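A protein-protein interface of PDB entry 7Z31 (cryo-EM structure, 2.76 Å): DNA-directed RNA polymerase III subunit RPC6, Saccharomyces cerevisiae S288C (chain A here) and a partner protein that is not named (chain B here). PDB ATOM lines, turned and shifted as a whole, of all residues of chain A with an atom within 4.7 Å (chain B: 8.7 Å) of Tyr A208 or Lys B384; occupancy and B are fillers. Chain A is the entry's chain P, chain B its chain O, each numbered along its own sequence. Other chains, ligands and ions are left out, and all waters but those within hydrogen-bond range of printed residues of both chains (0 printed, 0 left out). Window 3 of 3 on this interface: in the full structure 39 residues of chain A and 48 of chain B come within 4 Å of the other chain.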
ATOM      1  N   ASN A 189     -16.911   8.572  14.795  1.00  0.00           N
ATOM      2  CA  ASN A 189     -16.135   8.405  16.016  1.00  0.00           C
ATOM      3  C   ASN A 189     -16.978   8.108  17.244  1.00  0.00           C
ATOM      4  O   ASN A 189     -16.437   7.572  18.220  1.00  0.00           O
ATOM      5  CB  ASN A 189     -15.288   9.657  16.288  1.00  0.00           C
ATOM      6  CG  ASN A 189     -14.073   9.364  17.136  1.00  0.00           C
ATOM      7  OD1 ASN A 189     -13.022   8.980  16.623  1.00  0.00           O
ATOM      8  ND2 ASN A 189     -14.206   9.545  18.443  1.00  0.00           N
ATOM      9  N   THR A 190     -18.271   8.431  17.236  1.00  0.00           N
ATOM     10  CA  THR A 190     -19.170   8.145  18.347  1.00  0.00           C
ATOM     11  C   THR A 190     -20.047   6.924  18.098  1.00  0.00           C
ATOM     12  O   THR A 190     -20.267   6.126  19.016  1.00  0.00           O
ATOM     13  CB  THR A 190     -20.048   9.368  18.638  1.00  0.00           C
ATOM     14  OG1 THR A 190     -19.263  10.381  19.282  1.00  0.00           O
ATOM     15  CG2 THR A 190     -21.210   9.004  19.530  1.00  0.00           C
ATOM     16  N   PHE A 191     -20.552   6.754  16.879  1.00  0.00           N
ATOM     17  CA  PHE A 191     -21.246   5.526  16.533  1.00  0.00           C
ATOM     18  C   PHE A 191     -20.255   4.364  16.472  1.00  0.00           C
ATOM     19  O   PHE A 191     -19.080   4.559  16.150  1.00  0.00           O
ATOM     20  CB  PHE A 191     -21.964   5.671  15.195  1.00  0.00           C
ATOM     21  CG  PHE A 191     -23.455   5.809  15.321  1.00  0.00           C
ATOM     22  CD1 PHE A 191     -24.034   7.053  15.526  1.00  0.00           C
ATOM     23  CD2 PHE A 191     -24.277   4.698  15.234  1.00  0.00           C
ATOM     24  CE1 PHE A 191     -25.404   7.183  15.642  1.00  0.00           C
ATOM     25  CE2 PHE A 191     -25.648   4.822  15.349  1.00  0.00           C
ATOM     26  CZ  PHE A 191     -26.214   6.066  15.554  1.00  0.00           C
ATOM     27  N   PRO A 192     -20.705   3.144  16.789  1.00  0.00           N
ATOM     28  CA  PRO A 192     -19.765   2.010  16.838  1.00  0.00           C
ATOM     29  C   PRO A 192     -19.004   1.777  15.546  1.00  0.00           C
ATOM     30  O   PRO A 192     -17.812   1.449  15.586  1.00  0.00           O
ATOM     31  CB  PRO A 192     -20.678   0.821  17.171  1.00  0.00           C
ATOM     32  CG  PRO A 192     -21.842   1.429  17.885  1.00  0.00           C
ATOM     33  CD  PRO A 192     -22.057   2.767  17.242  1.00  0.00           C
ATOM     34  N   VAL A 206     -26.403  -1.201  15.912  1.00  0.00           N
ATOM     35  CA  VAL A 206     -26.160  -1.364  17.341  1.00  0.00           C
ATOM     36  C   VAL A 206     -25.985  -0.009  18.013  1.00  0.00           C
ATOM     37  O   VAL A 206     -25.683   0.999  17.373  1.00  0.00           O
ATOM     38  CB  VAL A 206     -24.923  -2.245  17.623  1.00  0.00           C
ATOM     39  CG1 VAL A 206     -25.221  -3.702  17.304  1.00  0.00           C
ATOM     40  CG2 VAL A 206     -23.730  -1.746  16.827  1.00  0.00           C
ATOM     41  N   PHE A 207     -26.182  -0.007  19.332  1.00  0.00           N
ATOM     42  CA  PHE A 207     -25.888   1.126  20.196  1.00  0.00           C
ATOM     43  C   PHE A 207     -24.851   0.706  21.227  1.00  0.00           C
ATOM     44  O   PHE A 207     -24.669  -0.481  21.513  1.00  0.00           O
ATOM     45  CB  PHE A 207     -27.150   1.655  20.894  1.00  0.00           C
ATOM     46  CG  PHE A 207     -27.789   2.817  20.192  1.00  0.00           C
ATOM     47  CD1 PHE A 207     -27.087   3.541  19.241  1.00  0.00           C
ATOM     48  CD2 PHE A 207     -29.086   3.193  20.487  1.00  0.00           C
ATOM     49  CE1 PHE A 207     -27.670   4.611  18.597  1.00  0.00           C
ATOM     50  CE2 PHE A 207     -29.672   4.267  19.845  1.00  0.00           C
ATOM     51  CZ  PHE A 207     -28.963   4.974  18.898  1.00  0.00           C
ATOM     52  N   TYR A 208     -24.164   1.698  21.785  1.00  0.00           N
ATOM     53  CA  TYR A 208     -23.103   1.454  22.749  1.00  0.00           C
ATOM     54  C   TYR A 208     -23.674   1.229  24.148  1.00  0.00           C
ATOM     55  O   TYR A 208     -24.857   1.451  24.414  1.00  0.00           O
ATOM     56  CB  TYR A 208     -22.112   2.618  22.765  1.00  0.00           C
ATOM     57  CG  TYR A 208     -20.923   2.443  21.844  1.00  0.00           C
ATOM     58  CD1 TYR A 208     -20.632   1.214  21.274  1.00  0.00           C
ATOM     59  CD2 TYR A 208     -20.086   3.510  21.558  1.00  0.00           C
ATOM     60  CE1 TYR A 208     -19.542   1.059  20.433  1.00  0.00           C
ATOM     61  CE2 TYR A 208     -18.999   3.367  20.727  1.00  0.00           C
ATOM     62  CZ  TYR A 208     -18.728   2.140  20.167  1.00  0.00           C
ATOM     63  OH  TYR A 208     -17.642   2.000  19.332  1.00  0.00           O
ATOM     64  N   ALA A 209     -22.802   0.779  25.053  1.00  0.00           N
ATOM     65  CA  ALA A 209     -23.177   0.524  26.434  1.00  0.00           C
ATOM     66  C   ALA A 209     -23.340   1.838  27.200  1.00  0.00           C
ATOM     67  O   ALA A 209     -22.746   2.857  26.834  1.00  0.00           O
ATOM     68  CB  ALA A 209     -22.127  -0.347  27.117  1.00  0.00           C
ATOM     69  N   PRO A 210     -24.166   1.848  28.251  1.00  0.00           N
ATOM     70  CA  PRO A 210     -24.349   3.092  29.019  1.00  0.00           C
ATOM     71  C   PRO A 210     -23.078   3.613  29.673  1.00  0.00           C
ATOM     72  O   PRO A 210     -22.902   4.834  29.767  1.00  0.00           O
ATOM     73  CB  PRO A 210     -25.402   2.700  30.066  1.00  0.00           C
ATOM     74  CG  PRO A 210     -25.298   1.207  30.169  1.00  0.00           C
ATOM     75  CD  PRO A 210     -24.995   0.752  28.779  1.00  0.00           C
ATOM     76  N   VAL A 212     -19.836   3.318  28.797  1.00  0.00           N
ATOM     77  CA  VAL A 212     -18.666   3.557  27.961  1.00  0.00           C
ATOM     78  C   VAL A 212     -18.605   5.035  27.591  1.00  0.00           C
ATOM     79  O   VAL A 212     -19.614   5.748  27.593  1.00  0.00           O
ATOM     80  CB  VAL A 212     -18.683   2.665  26.700  1.00  0.00           C
ATOM     81  CG1 VAL A 212     -19.709   3.172  25.699  1.00  0.00           C
ATOM     82  CG2 VAL A 212     -17.294   2.576  26.073  1.00  0.00           C
ATOM     83  N   ASN A 214     -18.679   6.897  24.869  1.00  0.00           N
ATOM     84  CA  ASN A 214     -19.046   6.852  23.459  1.00  0.00           C
ATOM     85  C   ASN A 214     -18.911   8.203  22.772  1.00  0.00           C
ATOM     86  O   ASN A 214     -18.908   8.257  21.539  1.00  0.00           O
ATOM     87  CB  ASN A 214     -20.485   6.350  23.310  1.00  0.00           C
ATOM     88  CG  ASN A 214     -21.466   7.122  24.174  1.00  0.00           C
ATOM     89  OD1 ASN A 214     -21.141   7.525  25.291  1.00  0.00           O
ATOM     90  ND2 ASN A 214     -22.677   7.329  23.661  1.00  0.00           N
ATOM     91  N   THR B 308     -32.837  -1.348  19.674  1.00  0.00           N
ATOM     92  CA  THR B 308     -33.170  -1.044  21.056  1.00  0.00           C
ATOM     93  C   THR B 308     -34.427  -0.191  21.179  1.00  0.00           C
ATOM     94  O   THR B 308     -34.797   0.185  22.293  1.00  0.00           O
ATOM     95  CB  THR B 308     -31.989  -0.348  21.741  1.00  0.00           C
ATOM     96  OG1 THR B 308     -32.192  -0.336  23.160  1.00  0.00           O
ATOM     97  CG2 THR B 308     -31.844   1.076  21.236  1.00  0.00           C
ATOM     98  N   GLY B 378     -28.387  -8.741  20.860  1.00  0.00           N
ATOM     99  CA  GLY B 378     -27.497  -7.892  20.100  1.00  0.00           C
ATOM    100  C   GLY B 378     -27.748  -6.409  20.245  1.00  0.00           C
ATOM    101  O   GLY B 378     -27.262  -5.624  19.424  1.00  0.00           O
ATOM    102  N   SER B 379     -28.489  -5.996  21.270  1.00  0.00           N
ATOM    103  CA  SER B 379     -28.864  -4.600  21.440  1.00  0.00           C
ATOM    104  C   SER B 379     -27.827  -3.785  22.199  1.00  0.00           C
ATOM    105  O   SER B 379     -28.153  -2.690  22.673  1.00  0.00           O
ATOM    106  CB  SER B 379     -30.210  -4.505  22.158  1.00  0.00           C
ATOM    107  OG  SER B 379     -30.556  -3.153  22.385  1.00  0.00           O
ATOM    108  N   LEU B 380     -26.600  -4.279  22.334  1.00  0.00           N
ATOM    109  CA  LEU B 380     -25.571  -3.584  23.093  1.00  0.00           C
ATOM    110  C   LEU B 380     -24.192  -3.921  22.545  1.00  0.00           C
ATOM    111  O   LEU B 380     -24.003  -4.913  21.838  1.00  0.00           O
ATOM    112  CB  LEU B 380     -25.636  -3.936  24.587  1.00  0.00           C
ATOM    113  CG  LEU B 380     -24.945  -5.233  25.015  1.00  0.00           C
ATOM    114  CD1 LEU B 380     -24.786  -5.291  26.526  1.00  0.00           C
ATOM    115  CD2 LEU B 380     -25.689  -6.461  24.506  1.00  0.00           C
ATOM    116  N   LEU B 381     -23.227  -3.072  22.891  1.00  0.00           N
ATOM    117  CA  LEU B 381     -21.824  -3.272  22.536  1.00  0.00           C
ATOM    118  C   LEU B 381     -20.980  -2.753  23.692  1.00  0.00           C
ATOM    119  O   LEU B 381     -20.831  -1.538  23.856  1.00  0.00           O
ATOM    120  CB  LEU B 381     -21.476  -2.561  21.227  1.00  0.00           C
ATOM    121  CG  LEU B 381     -20.083  -2.790  20.637  1.00  0.00           C
ATOM    122  CD1 LEU B 381     -19.707  -4.261  20.679  1.00  0.00           C
ATOM    123  CD2 LEU B 381     -20.029  -2.271  19.212  1.00  0.00           C
ATOM    124  N   SER B 382     -20.427  -3.678  24.493  1.00  0.00           N
ATOM    125  CA  SER B 382     -19.700  -3.427  25.743  1.00  0.00           C
ATOM    126  C   SER B 382     -18.346  -2.776  25.545  1.00  0.00           C
ATOM    127  O   SER B 382     -17.597  -2.659  26.528  1.00  0.00           O
ATOM    128  CB  SER B 382     -19.523  -4.739  26.512  1.00  0.00           C
ATOM    129  OG  SER B 382     -18.563  -4.601  27.547  1.00  0.00           O
ATOM    130  N   ARG B 383     -17.999  -2.362  24.333  1.00  0.00           N
ATOM    131  CA  ARG B 383     -16.724  -1.715  24.057  1.00  0.00           C
ATOM    132  C   ARG B 383     -16.854  -0.986  22.726  1.00  0.00           C
ATOM    133  O   ARG B 383     -17.962  -0.805  22.208  1.00  0.00           O
ATOM    134  CB  ARG B 383     -15.579  -2.732  24.053  1.00  0.00           C
ATOM    135  CG  ARG B 383     -15.964  -4.101  23.526  1.00  0.00           C
ATOM    136  CD  ARG B 383     -14.810  -5.077  23.685  1.00  0.00           C
ATOM    137  NE  ARG B 383     -14.338  -5.116  25.063  1.00  0.00           N
ATOM    138  CZ  ARG B 383     -14.685  -6.038  25.948  1.00  0.00           C
ATOM    139  NH1 ARG B 383     -15.481  -7.044  25.621  1.00  0.00           N
ATOM    140  NH2 ARG B 383     -14.222  -5.952  27.191  1.00  0.00           N
ATOM    141  N   LYS B 384     -15.723  -0.558  22.175  1.00  0.00           N
ATOM    142  CA  LYS B 384     -15.714   0.075  20.863  1.00  0.00           C
ATOM    143  C   LYS B 384     -15.749  -0.979  19.764  1.00  0.00           C
ATOM    144  O   LYS B 384     -16.711  -1.739  19.657  1.00  0.00           O
ATOM    145  CB  LYS B 384     -14.492   0.979  20.699  1.00  0.00           C
ATOM    146  CG  LYS B 384     -14.744   2.437  21.052  1.00  0.00           C
ATOM    147  CD  LYS B 384     -13.470   3.261  20.975  1.00  0.00           C
ATOM    148  CE  LYS B 384     -13.735   4.741  21.216  1.00  0.00           C
ATOM    149  NZ  LYS B 384     -14.474   5.384  20.091  1.00  0.00           N
ATOM    150  N   LEU B 452     -29.398  -6.918  30.553  1.00  0.00           N
ATOM    151  CA  LEU B 452     -29.462  -6.232  29.270  1.00  0.00           C
ATOM    152  C   LEU B 452     -30.675  -5.315  29.152  1.00  0.00           C
ATOM    153  O   LEU B 452     -30.567  -4.236  28.556  1.00  0.00           O
ATOM    154  CB  LEU B 452     -29.459  -7.255  28.130  1.00  0.00           C
ATOM    155  CG  LEU B 452     -29.248  -6.760  26.695  1.00  0.00           C
ATOM    156  CD1 LEU B 452     -30.573  -6.486  26.003  1.00  0.00           C
ATOM    157  CD2 LEU B 452     -28.363  -5.523  26.680  1.00  0.00           C
ATOM    158  N   SER B 455     -29.876  -2.435  31.029  1.00  0.00           N
ATOM    159  CA  SER B 455     -28.980  -1.584  30.253  1.00  0.00           C
ATOM    160  C   SER B 455     -29.768  -0.547  29.465  1.00  0.00           C
ATOM    161  O   SER B 455     -29.407   0.636  29.447  1.00  0.00           O
ATOM    162  CB  SER B 455     -28.118  -2.432  29.318  1.00  0.00           C
ATOM    163  OG  SER B 455     -27.292  -1.615  28.508  1.00  0.00           O
ATOM    164  N   HIS B 456     -30.861  -0.968  28.822  1.00  0.00           N
ATOM    165  CA  HIS B 456     -31.712  -0.023  28.105  1.00  0.00           C
ATOM    166  C   HIS B 456     -32.420   0.925  29.067  1.00  0.00           C
ATOM    167  O   HIS B 456     -32.594   2.109  28.761  1.00  0.00           O
ATOM    168  CB  HIS B 456     -32.725  -0.773  27.243  1.00  0.00           C
ATOM    169  CG  HIS B 456     -32.103  -1.761  26.307  1.00  0.00           C
ATOM    170  ND1 HIS B 456     -32.802  -2.825  25.781  1.00  0.00           N
ATOM    171  CD2 HIS B 456     -30.849  -1.848  25.802  1.00  0.00           C
ATOM    172  CE1 HIS B 456     -32.005  -3.528  24.995  1.00  0.00           C
ATOM    173  NE2 HIS B 456     -30.815  -2.955  24.989  1.00  0.00           N
ATOM    174  N   ILE B 459     -29.742   3.475  29.903  1.00  0.00           N
ATOM    175  CA  ILE B 459     -29.400   4.346  28.782  1.00  0.00           C
ATOM    176  C   ILE B 459     -30.543   5.310  28.478  1.00  0.00           C
ATOM    177  O   ILE B 459     -30.304   6.460  28.093  1.00  0.00           O
ATOM    178  CB  ILE B 459     -28.983   3.531  27.542  1.00  0.00           C
ATOM    179  CG1 ILE B 459     -28.233   4.428  26.554  1.00  0.00           C
ATOM    180  CG2 ILE B 459     -30.181   2.915  26.841  1.00  0.00           C
ATOM    181  CD1 ILE B 459     -27.020   5.095  27.142  1.00  0.00           C
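The side-chain hydroxyl (OG1) of Thr B308 lies close to the side-chain hydroxyl (OG) of Ser B379 (3.3 Å). The side-chain hydroxyl (OG1) of Thr B308 lies close to a ring nitrogen (NE2) of His B456, 3.5 Å away.
Printed residues of chain B within 4 Å of Val A206: Gly B378 (3.5 Å). Tyr A208 touches just these residues of chain B: Leu B381 (3.6 Å), Arg B383 (3.0 Å) and Lys B384 (3.1 Å). Ala A209 touches just one residue of chain B: Leu B381 (3.3 Å). Printed residues of chain B within 4 Å of Pro A210: Ser B455 and Ile B459. Printed residues of chain A within 4 Å of Thr B308: Phe A207. Of the printed residues of chain A, Leu B380 touches Phe A207. Of the printed residues of chain A, Leu B381 touches Pro A192 (3.8 Å), Phe A207 (3.3 Å), Tyr A208 (3.6 Å) and Ala A209 (3.3 Å). Lys B384 touches just these residues of chain A: Asn A189 and Tyr A208. The nearest residue of chain B that does not touch Tyr A208 is Ile B459 (5.0 Å). The nearest printed residue of chain A that does not touch Lys B384 is Val A212 (5.2 Å). The nearest printed residue of chain A that does not touch Leu B380 is Val A206 (4.8 Å).
The backbone NH (N) of Leu B381 is in hydrogen-bond range of the backbone carbonyl oxygen (O) of Phe A207, 3.3 Å away. The backbone carbonyl oxygen (O) of Leu B381 is in hydrogen-bond range of the backbone NH (N) of Ala A209, 3.3 Å away. The side-chain amino group (NZ) of Lys B384 is in hydrogen-bond range of the backbone carbonyl oxygen (O) of Asn A189 (3.5 Å).
Among the printed residues, pairs that only touch across the chains: Pro A192 with Leu B381 (3.8 Å), Val A206 with Gly B378 (3.5 Å), Phe A207 with Thr B308 (3.6 Å), Phe A207 with Leu B380 (3.6 Å), Tyr A208 with Leu B381 (3.6 Å), Tyr A208 with Arg B383 (3.0 Å), Tyr A208 with Lys B384 (3.1 Å), Pro A210 with Ser B455 (3.3 Å) and Pro A210 with Ile B459 (3.8 Å).
Hydrophobic or aromatic side chains of chain A within 4 Å of the printed part of chain B: Pro A192, Val A206, Phe A207, Tyr A208, Ala A209 and Pro A210. Printed residues of chain B that touch a printed residue of chain A: Thr B308, Gly B378, Leu B380, Leu B381, Arg B383, Lys B384, Ser B455 and Ile B459. Hydrophobic or aromatic side chains of chain B within 4 Å of the printed part of chain A: Leu B381 and Ile B459. Among the printed residues, 12 pairs touch across the chains.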
